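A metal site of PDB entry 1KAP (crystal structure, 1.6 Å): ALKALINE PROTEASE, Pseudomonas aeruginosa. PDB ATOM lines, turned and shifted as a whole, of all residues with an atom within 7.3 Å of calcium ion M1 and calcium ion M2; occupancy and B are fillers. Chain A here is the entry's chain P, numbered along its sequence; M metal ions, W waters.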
ATOM      1  N   LEU A 314      -1.775 -27.452  -5.835  1.00  0.00           N
ATOM      2  CA  LEU A 314      -2.875 -28.389  -5.617  1.00  0.00           C
ATOM      3  C   LEU A 314      -4.229 -28.019  -6.230  1.00  0.00           C
ATOM      4  O   LEU A 314      -5.198 -28.749  -6.052  1.00  0.00           O
ATOM      5  CB  LEU A 314      -3.057 -28.703  -4.129  1.00  0.00           C
ATOM      6  CG  LEU A 314      -1.924 -29.404  -3.375  1.00  0.00           C
ATOM      7  CD1 LEU A 314      -2.376 -29.661  -1.939  1.00  0.00           C
ATOM      8  CD2 LEU A 314      -1.535 -30.730  -4.053  1.00  0.00           C
ATOM      9  N   GLU A 338      -5.692 -33.253  -1.448  1.00  0.00           N
ATOM     10  CA  GLU A 338      -5.562 -32.560  -0.177  1.00  0.00           C
ATOM     11  C   GLU A 338      -4.201 -32.182   0.355  1.00  0.00           C
ATOM     12  O   GLU A 338      -4.038 -31.114   0.945  1.00  0.00           O
ATOM     13  CB  GLU A 338      -6.286 -33.367   0.916  1.00  0.00           C
ATOM     14  CG  GLU A 338      -7.806 -33.468   0.788  1.00  0.00           C
ATOM     15  CD  GLU A 338      -8.314 -34.395  -0.322  1.00  0.00           C
ATOM     16  OE1 GLU A 338      -7.544 -35.216  -0.874  1.00  0.00           O
ATOM     17  OE2 GLU A 338      -9.515 -34.306  -0.643  1.00  0.00           O
ATOM     18  N   ILE A 350       1.659 -24.722  -2.994  1.00  0.00           N
ATOM     19  CA  ILE A 350       0.425 -23.945  -3.047  1.00  0.00           C
ATOM     20  C   ILE A 350      -0.769 -24.869  -2.823  1.00  0.00           C
ATOM     21  O   ILE A 350      -0.997 -25.814  -3.583  1.00  0.00           O
ATOM     22  CB  ILE A 350       0.300 -23.241  -4.425  1.00  0.00           C
ATOM     23  CG1 ILE A 350       1.456 -22.238  -4.618  1.00  0.00           C
ATOM     24  CG2 ILE A 350      -1.070 -22.569  -4.573  1.00  0.00           C
ATOM     25  CD1 ILE A 350       1.476 -21.565  -5.968  1.00  0.00           C
ATOM     26  N   GLY A 351      -1.494 -24.601  -1.740  1.00  0.00           N
ATOM     27  CA  GLY A 351      -2.673 -25.395  -1.412  1.00  0.00           C
ATOM     28  C   GLY A 351      -3.883 -24.909  -2.191  1.00  0.00           C
ATOM     29  O   GLY A 351      -3.802 -23.983  -3.005  1.00  0.00           O
ATOM     30  N   ASN A 352      -5.027 -25.535  -1.953  1.00  0.00           N
ATOM     31  CA  ASN A 352      -6.254 -25.174  -2.624  1.00  0.00           C
ATOM     32  C   ASN A 352      -7.276 -24.713  -1.582  1.00  0.00           C
ATOM     33  O   ASN A 352      -6.912 -24.429  -0.455  1.00  0.00           O
ATOM     34  CB  ASN A 352      -6.772 -26.331  -3.500  1.00  0.00           C
ATOM     35  CG  ASN A 352      -6.913 -27.618  -2.732  1.00  0.00           C
ATOM     36  OD1 ASN A 352      -7.170 -27.634  -1.534  1.00  0.00           O
ATOM     37  ND2 ASN A 352      -6.717 -28.736  -3.423  1.00  0.00           N
ATOM     38  N   ASP A 353      -8.549 -24.662  -1.962  1.00  0.00           N
ATOM     39  CA  ASP A 353      -9.596 -24.173  -1.062  1.00  0.00           C
ATOM     40  C   ASP A 353      -9.950 -25.003   0.157  1.00  0.00           C
ATOM     41  O   ASP A 353     -10.662 -24.506   1.039  1.00  0.00           O
ATOM     42  CB  ASP A 353     -10.878 -23.906  -1.844  1.00  0.00           C
ATOM     43  CG  ASP A 353     -10.739 -22.796  -2.880  1.00  0.00           C
ATOM     44  OD1 ASP A 353      -9.676 -22.127  -2.940  1.00  0.00           O
ATOM     45  OD2 ASP A 353     -11.726 -22.592  -3.637  1.00  0.00           O
ATOM     46  N   VAL A 354      -9.544 -26.264   0.207  1.00  0.00           N
ATOM     47  CA  VAL A 354      -9.874 -27.106   1.348  1.00  0.00           C
ATOM     48  C   VAL A 354      -8.719 -27.137   2.339  1.00  0.00           C
ATOM     49  O   VAL A 354      -7.661 -26.566   2.079  1.00  0.00           O
ATOM     50  CB  VAL A 354     -10.270 -28.572   0.920  1.00  0.00           C
ATOM     51  CG1 VAL A 354     -11.424 -28.514  -0.091  1.00  0.00           C
ATOM     52  CG2 VAL A 354      -9.070 -29.352   0.349  1.00  0.00           C
ATOM     53  N   ALA A 355      -8.922 -27.792   3.478  1.00  0.00           N
ATOM     54  CA  ALA A 355      -7.870 -27.915   4.481  1.00  0.00           C
ATOM     55  C   ALA A 355      -6.783 -28.835   3.905  1.00  0.00           C
ATOM     56  O   ALA A 355      -7.062 -29.989   3.537  1.00  0.00           O
ATOM     57  CB  ALA A 355      -8.426 -28.509   5.761  1.00  0.00           C
ATOM     58  N   ASN A 356      -5.570 -28.313   3.799  1.00  0.00           N
ATOM     59  CA  ASN A 356      -4.442 -29.073   3.244  1.00  0.00           C
ATOM     60  C   ASN A 356      -3.350 -29.291   4.276  1.00  0.00           C
ATOM     61  O   ASN A 356      -3.186 -28.464   5.180  1.00  0.00           O
ATOM     62  CB  ASN A 356      -3.758 -28.288   2.112  1.00  0.00           C
ATOM     63  CG  ASN A 356      -4.713 -27.806   1.085  1.00  0.00           C
ATOM     64  OD1 ASN A 356      -4.831 -26.610   0.845  1.00  0.00           O
ATOM     65  ND2 ASN A 356      -5.395 -28.735   0.427  1.00  0.00           N
ATOM     66  N   VAL A 357      -2.603 -30.375   4.118  1.00  0.00           N
ATOM     67  CA  VAL A 357      -1.433 -30.630   4.947  1.00  0.00           C
ATOM     68  C   VAL A 357      -0.312 -30.432   3.920  1.00  0.00           C
ATOM     69  O   VAL A 357      -0.293 -31.118   2.899  1.00  0.00           O
ATOM     70  CB  VAL A 357      -1.327 -32.078   5.492  1.00  0.00           C
ATOM     71  CG1 VAL A 357       0.036 -32.300   6.160  1.00  0.00           C
ATOM     72  CG2 VAL A 357      -2.428 -32.334   6.500  1.00  0.00           C
ATOM     73  N   LEU A 358       0.525 -29.419   4.126  1.00  0.00           N
ATOM     74  CA  LEU A 358       1.636 -29.118   3.232  1.00  0.00           C
ATOM     75  C   LEU A 358       2.923 -29.262   4.055  1.00  0.00           C
ATOM     76  O   LEU A 358       3.035 -28.673   5.126  1.00  0.00           O
ATOM     77  CB  LEU A 358       1.546 -27.688   2.684  1.00  0.00           C
ATOM     78  CG  LEU A 358       0.278 -27.324   1.911  1.00  0.00           C
ATOM     79  CD1 LEU A 358       0.350 -25.869   1.480  1.00  0.00           C
ATOM     80  CD2 LEU A 358       0.137 -28.237   0.698  1.00  0.00           C
ATOM     81  N   TYR A 368       1.893 -21.792   0.885  1.00  0.00           N
ATOM     82  CA  TYR A 368       0.711 -20.953   0.772  1.00  0.00           C
ATOM     83  C   TYR A 368      -0.508 -21.865   0.935  1.00  0.00           C
ATOM     84  O   TYR A 368      -0.879 -22.581   0.009  1.00  0.00           O
ATOM     85  CB  TYR A 368       0.697 -20.309  -0.603  1.00  0.00           C
ATOM     86  CG  TYR A 368      -0.410 -19.319  -0.817  1.00  0.00           C
ATOM     87  CD1 TYR A 368      -0.209 -17.971  -0.518  1.00  0.00           C
ATOM     88  CD2 TYR A 368      -1.643 -19.701  -1.354  1.00  0.00           C
ATOM     89  CE1 TYR A 368      -1.185 -17.024  -0.755  1.00  0.00           C
ATOM     90  CE2 TYR A 368      -2.639 -18.760  -1.601  1.00  0.00           C
ATOM     91  CZ  TYR A 368      -2.398 -17.414  -1.297  1.00  0.00           C
ATOM     92  OH  TYR A 368      -3.313 -16.437  -1.580  1.00  0.00           O
ATOM     93  N   GLY A 369      -1.117 -21.861   2.118  1.00  0.00           N
ATOM     94  CA  GLY A 369      -2.255 -22.738   2.342  1.00  0.00           C
ATOM     95  C   GLY A 369      -3.538 -22.419   1.583  1.00  0.00           C
ATOM     96  O   GLY A 369      -4.315 -23.329   1.283  1.00  0.00           O
ATOM     97  N   GLY A 370      -3.752 -21.135   1.268  1.00  0.00           N
ATOM     98  CA  GLY A 370      -4.981 -20.737   0.605  1.00  0.00           C
ATOM     99  C   GLY A 370      -6.155 -20.821   1.583  1.00  0.00           C
ATOM    100  O   GLY A 370      -5.955 -20.782   2.803  1.00  0.00           O
ATOM    101  N   LEU A 371      -7.375 -20.941   1.080  1.00  0.00           N
ATOM    102  CA  LEU A 371      -8.523 -21.041   1.970  1.00  0.00           C
ATOM    103  C   LEU A 371      -8.494 -22.327   2.790  1.00  0.00           C
ATOM    104  O   LEU A 371      -7.767 -23.268   2.470  1.00  0.00           O
ATOM    105  CB  LEU A 371      -9.838 -20.932   1.179  1.00  0.00           C
ATOM    106  CG  LEU A 371     -10.117 -19.630   0.409  1.00  0.00           C
ATOM    107  CD1 LEU A 371     -11.433 -19.748  -0.331  1.00  0.00           C
ATOM    108  CD2 LEU A 371     -10.157 -18.438   1.359  1.00  0.00           C
ATOM    109  N   GLY A 372      -9.312 -22.367   3.847  1.00  0.00           N
ATOM    110  CA  GLY A 372      -9.362 -23.520   4.716  1.00  0.00           C
ATOM    111  C   GLY A 372      -8.332 -23.442   5.835  1.00  0.00           C
ATOM    112  O   GLY A 372      -7.415 -22.638   5.794  1.00  0.00           O
ATOM    113  N   ALA A 373      -8.532 -24.244   6.868  1.00  0.00           N
ATOM    114  CA  ALA A 373      -7.615 -24.286   8.008  1.00  0.00           C
ATOM    115  C   ALA A 373      -6.520 -25.300   7.661  1.00  0.00           C
ATOM    116  O   ALA A 373      -6.682 -26.515   7.843  1.00  0.00           O
ATOM    117  CB  ALA A 373      -8.357 -24.735   9.256  1.00  0.00           C
ATOM    118  N   ASP A 374      -5.396 -24.796   7.165  1.00  0.00           N
ATOM    119  CA  ASP A 374      -4.302 -25.674   6.757  1.00  0.00           C
ATOM    120  C   ASP A 374      -3.309 -25.999   7.859  1.00  0.00           C
ATOM    121  O   ASP A 374      -3.127 -25.208   8.779  1.00  0.00           O
ATOM    122  CB  ASP A 374      -3.600 -25.030   5.550  1.00  0.00           C
ATOM    123  CG  ASP A 374      -4.581 -24.616   4.459  1.00  0.00           C
ATOM    124  OD1 ASP A 374      -5.174 -25.514   3.821  1.00  0.00           O
ATOM    125  OD2 ASP A 374      -4.816 -23.414   4.279  1.00  0.00           O
ATOM    126  N   GLN A 375      -2.698 -27.184   7.755  1.00  0.00           N
ATOM    127  CA  GLN A 375      -1.673 -27.674   8.697  1.00  0.00           C
ATOM    128  C   GLN A 375      -0.388 -27.532   7.913  1.00  0.00           C
ATOM    129  O   GLN A 375      -0.139 -28.316   6.977  1.00  0.00           O
ATOM    130  CB  GLN A 375      -1.898 -29.137   9.038  1.00  0.00           C
ATOM    131  CG  GLN A 375      -3.277 -29.426   9.575  1.00  0.00           C
ATOM    132  CD  GLN A 375      -3.588 -28.576  10.781  1.00  0.00           C
ATOM    133  OE1 GLN A 375      -2.845 -28.609  11.757  1.00  0.00           O
ATOM    134  NE2 GLN A 375      -4.642 -27.780  10.709  1.00  0.00           N
ATOM    135  N   LEU A 376       0.439 -26.568   8.297  1.00  0.00           N
ATOM    136  CA  LEU A 376       1.659 -26.271   7.577  1.00  0.00           C
ATOM    137  C   LEU A 376       2.937 -26.631   8.307  1.00  0.00           C
ATOM    138  O   LEU A 376       3.166 -26.188   9.435  1.00  0.00           O
ATOM    139  CB  LEU A 376       1.658 -24.792   7.172  1.00  0.00           C
ATOM    140  CG  LEU A 376       0.392 -24.295   6.468  1.00  0.00           C
ATOM    141  CD1 LEU A 376       0.481 -22.805   6.197  1.00  0.00           C
ATOM    142  CD2 LEU A 376       0.174 -25.070   5.153  1.00  0.00           C
ATOM    143  N   VAL A 386       3.122 -17.866   3.557  1.00  0.00           N
ATOM    144  CA  VAL A 386       2.542 -16.727   2.878  1.00  0.00           C
ATOM    145  C   VAL A 386       1.012 -16.628   2.911  1.00  0.00           C
ATOM    146  O   VAL A 386       0.304 -17.633   2.803  1.00  0.00           O
ATOM    147  CB  VAL A 386       3.057 -16.694   1.402  1.00  0.00           C
ATOM    148  CG1 VAL A 386       2.529 -15.512   0.638  1.00  0.00           C
ATOM    149  CG2 VAL A 386       4.589 -16.703   1.378  1.00  0.00           C
ATOM    150  N   TYR A 387       0.522 -15.392   3.064  1.00  0.00           N
ATOM    151  CA  TYR A 387      -0.918 -15.108   3.115  1.00  0.00           C
ATOM    152  C   TYR A 387      -1.269 -13.989   2.148  1.00  0.00           C
ATOM    153  O   TYR A 387      -0.577 -12.973   2.100  1.00  0.00           O
ATOM    154  CB  TYR A 387      -1.325 -14.731   4.537  1.00  0.00           C
ATOM    155  CG  TYR A 387      -1.180 -15.883   5.482  1.00  0.00           C
ATOM    156  CD1 TYR A 387       0.070 -16.180   6.036  1.00  0.00           C
ATOM    157  CD2 TYR A 387      -2.242 -16.752   5.712  1.00  0.00           C
ATOM    158  CE1 TYR A 387       0.249 -17.333   6.781  1.00  0.00           C
ATOM    159  CE2 TYR A 387      -2.070 -17.890   6.462  1.00  0.00           C
ATOM    160  CZ  TYR A 387      -0.822 -18.172   6.988  1.00  0.00           C
ATOM    161  OH  TYR A 387      -0.615 -19.342   7.679  1.00  0.00           O
ATOM    162  N   ALA A 391      -9.245 -14.095   4.656  1.00  0.00           N
ATOM    163  CA  ALA A 391     -10.080 -15.293   4.637  1.00  0.00           C
ATOM    164  C   ALA A 391      -9.289 -16.596   4.672  1.00  0.00           C
ATOM    165  O   ALA A 391      -9.828 -17.634   5.056  1.00  0.00           O
ATOM    166  CB  ALA A 391     -10.988 -15.282   3.413  1.00  0.00           C
ATOM    167  N   GLU A 392      -8.023 -16.521   4.275  1.00  0.00           N
ATOM    168  CA  GLU A 392      -7.173 -17.695   4.259  1.00  0.00           C
ATOM    169  C   GLU A 392      -6.851 -18.274   5.624  1.00  0.00           C
ATOM    170  O   GLU A 392      -6.483 -19.433   5.740  1.00  0.00           O
ATOM    171  CB  GLU A 392      -5.914 -17.391   3.467  1.00  0.00           C
ATOM    172  CG  GLU A 392      -6.242 -17.161   2.015  1.00  0.00           C
ATOM    173  CD  GLU A 392      -5.071 -16.682   1.223  1.00  0.00           C
ATOM    174  OE1 GLU A 392      -3.969 -16.527   1.775  1.00  0.00           O
ATOM    175  OE2 GLU A 392      -5.259 -16.443   0.020  1.00  0.00           O
ATOM    176  N   SER A 393      -6.980 -17.460   6.681  1.00  0.00           N
ATOM    177  CA  SER A 393      -6.738 -17.959   8.030  1.00  0.00           C
ATOM    178  C   SER A 393      -7.597 -17.099   8.943  1.00  0.00           C
ATOM    179  O   SER A 393      -7.102 -16.248   9.672  1.00  0.00           O
ATOM    180  CB  SER A 393      -5.256 -17.845   8.394  1.00  0.00           C
ATOM    181  OG  SER A 393      -4.976 -18.691   9.509  1.00  0.00           O
ATOM    182  N   SER A 394      -8.907 -17.299   8.844  1.00  0.00           N
ATOM    183  CA  SER A 394      -9.854 -16.534   9.643  1.00  0.00           C
ATOM    184  C   SER A 394      -9.792 -16.991  11.094  1.00  0.00           C
ATOM    185  O   SER A 394      -9.381 -18.116  11.395  1.00  0.00           O
ATOM    186  CB  SER A 394     -11.267 -16.730   9.102  1.00  0.00           C
ATOM    187  OG  SER A 394     -11.693 -18.062   9.319  1.00  0.00           O
ATOM    188  N   ALA A 397     -11.394 -20.394  11.616  1.00  0.00           N
ATOM    189  CA  ALA A 397     -10.752 -21.614  11.132  1.00  0.00           C
ATOM    190  C   ALA A 397      -9.304 -21.249  10.768  1.00  0.00           C
ATOM    191  O   ALA A 397      -8.956 -21.127   9.584  1.00  0.00           O
ATOM    192  CB  ALA A 397     -11.490 -22.159   9.919  1.00  0.00           C
ATOM    193  N   PRO A 398      -8.463 -21.060  11.781  1.00  0.00           N
ATOM    194  CA  PRO A 398      -7.070 -20.698  11.519  1.00  0.00           C
ATOM    195  C   PRO A 398      -6.155 -21.838  11.101  1.00  0.00           C
ATOM    196  O   PRO A 398      -6.387 -23.003  11.428  1.00  0.00           O
ATOM    197  CB  PRO A 398      -6.613 -20.111  12.856  1.00  0.00           C
ATOM    198  CG  PRO A 398      -7.358 -20.953  13.852  1.00  0.00           C
ATOM    199  CD  PRO A 398      -8.738 -21.085  13.238  1.00  0.00           C
ATOM    200  N   ASP A 399      -5.116 -21.483  10.361  1.00  0.00           N
ATOM    201  CA  ASP A 399      -4.104 -22.447   9.975  1.00  0.00           C
ATOM    202  C   ASP A 399      -3.338 -22.751  11.269  1.00  0.00           C
ATOM    203  O   ASP A 399      -3.425 -22.001  12.247  1.00  0.00           O
ATOM    204  CB  ASP A 399      -3.053 -21.791   9.083  1.00  0.00           C
ATOM    205  CG  ASP A 399      -3.512 -21.515   7.663  1.00  0.00           C
ATOM    206  OD1 ASP A 399      -4.625 -21.899   7.248  1.00  0.00           O
ATOM    207  OD2 ASP A 399      -2.692 -20.893   6.960  1.00  0.00           O
ATOM    208  N   THR A 400      -2.544 -23.801  11.232  1.00  0.00           N
ATOM    209  CA  THR A 400      -1.657 -24.120  12.342  1.00  0.00           C
ATOM    210  C   THR A 400      -0.282 -24.341  11.702  1.00  0.00           C
ATOM    211  O   THR A 400      -0.164 -25.134  10.765  1.00  0.00           O
ATOM    212  CB  THR A 400      -2.066 -25.378  13.111  1.00  0.00           C
ATOM    213  OG1 THR A 400      -3.341 -25.168  13.723  1.00  0.00           O
ATOM    214  CG2 THR A 400      -1.041 -25.673  14.206  1.00  0.00           C
HETATM  215 CA    CA M   1      -6.092 -24.761   1.766  1.00  0.00          CA
HETATM  216 CA    CA M   2      -5.489 -21.415   5.041  1.00  0.00          CA
HETATM  217  O   HOH W   1      -3.411 -20.356   4.493  1.00  0.00           O
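The side-chain amide nitrogen (ND2) of Asn 356 lies within hydrogen-bond range of the backbone carbonyl oxygen (O) of Glu 338.
OE2 of Glu 392 sits at hydrogen-bond distance from OH of Tyr 368 (2.5 Å).
OD1 of Asn 352 lies close to N of Val 354 (3.2 Å).
The backbone NH (N) of Thr 400 sits at hydrogen-bond distance from the backbone carbonyl oxygen (O) of Asp 374 (2.9 Å).
The backbone NH (N) of Gln 375 is in hydrogen-bond range of the backbone carbonyl oxygen (O) of Asn 356 (2.9 Å).
The backbone carbonyl oxygen (O) of Leu 314 is in hydrogen-bond range of the side-chain amide nitrogen (ND2) of Asn 352, at 3.0 Å.
OH of Tyr 387 lies within hydrogen-bond range of OD2 of Asp 399.
The backbone NH (N) of Asp 399 is in hydrogen-bond range of the side-chain hydroxyl (OG) of Ser 393.
Seven residues have an atom within 4 Å of calcium ion M1: Asn 352, Val 354, Asn 356, Gly 369, Gly 370, Leu 371 and Asp 374.
Six residues have an atom within 4 Å of calcium ion M2: Gly 370, Leu 371, Gly 372, Asp 374, Glu 392 and Asp 399.
Calcium ion M1 is bound by O of Gly 369 (2.3 Å), O of Leu 371 (2.4 Å), OD1 of Asp 374 (2.4 Å), O of Asn 352 (2.4 Å), O of Val 354 (2.4 Å) and OD1 of Asn 356 (2.4 Å).
Calcium ion M1 has six donor atoms within binding distance.
Slightly farther from calcium ion M1 lies the side-chain carboxylate (OD2) of Asp 374 (3.1 Å).
Calcium ion M2 is bound by the side-chain carboxylate of Asp 374, the backbone carbonyl oxygen of Glu 392, the backbone carbonyl oxygen of Gly 370, water W1, the backbone carbonyl oxygen of Gly 372 and the side-chain carboxylate of Asp 399.
Water W1 lies within hydrogen-bond range of the side-chain carboxylate of Asp 399 (2.6 Å) and the backbone NH of Gly 370 (3.3 Å).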
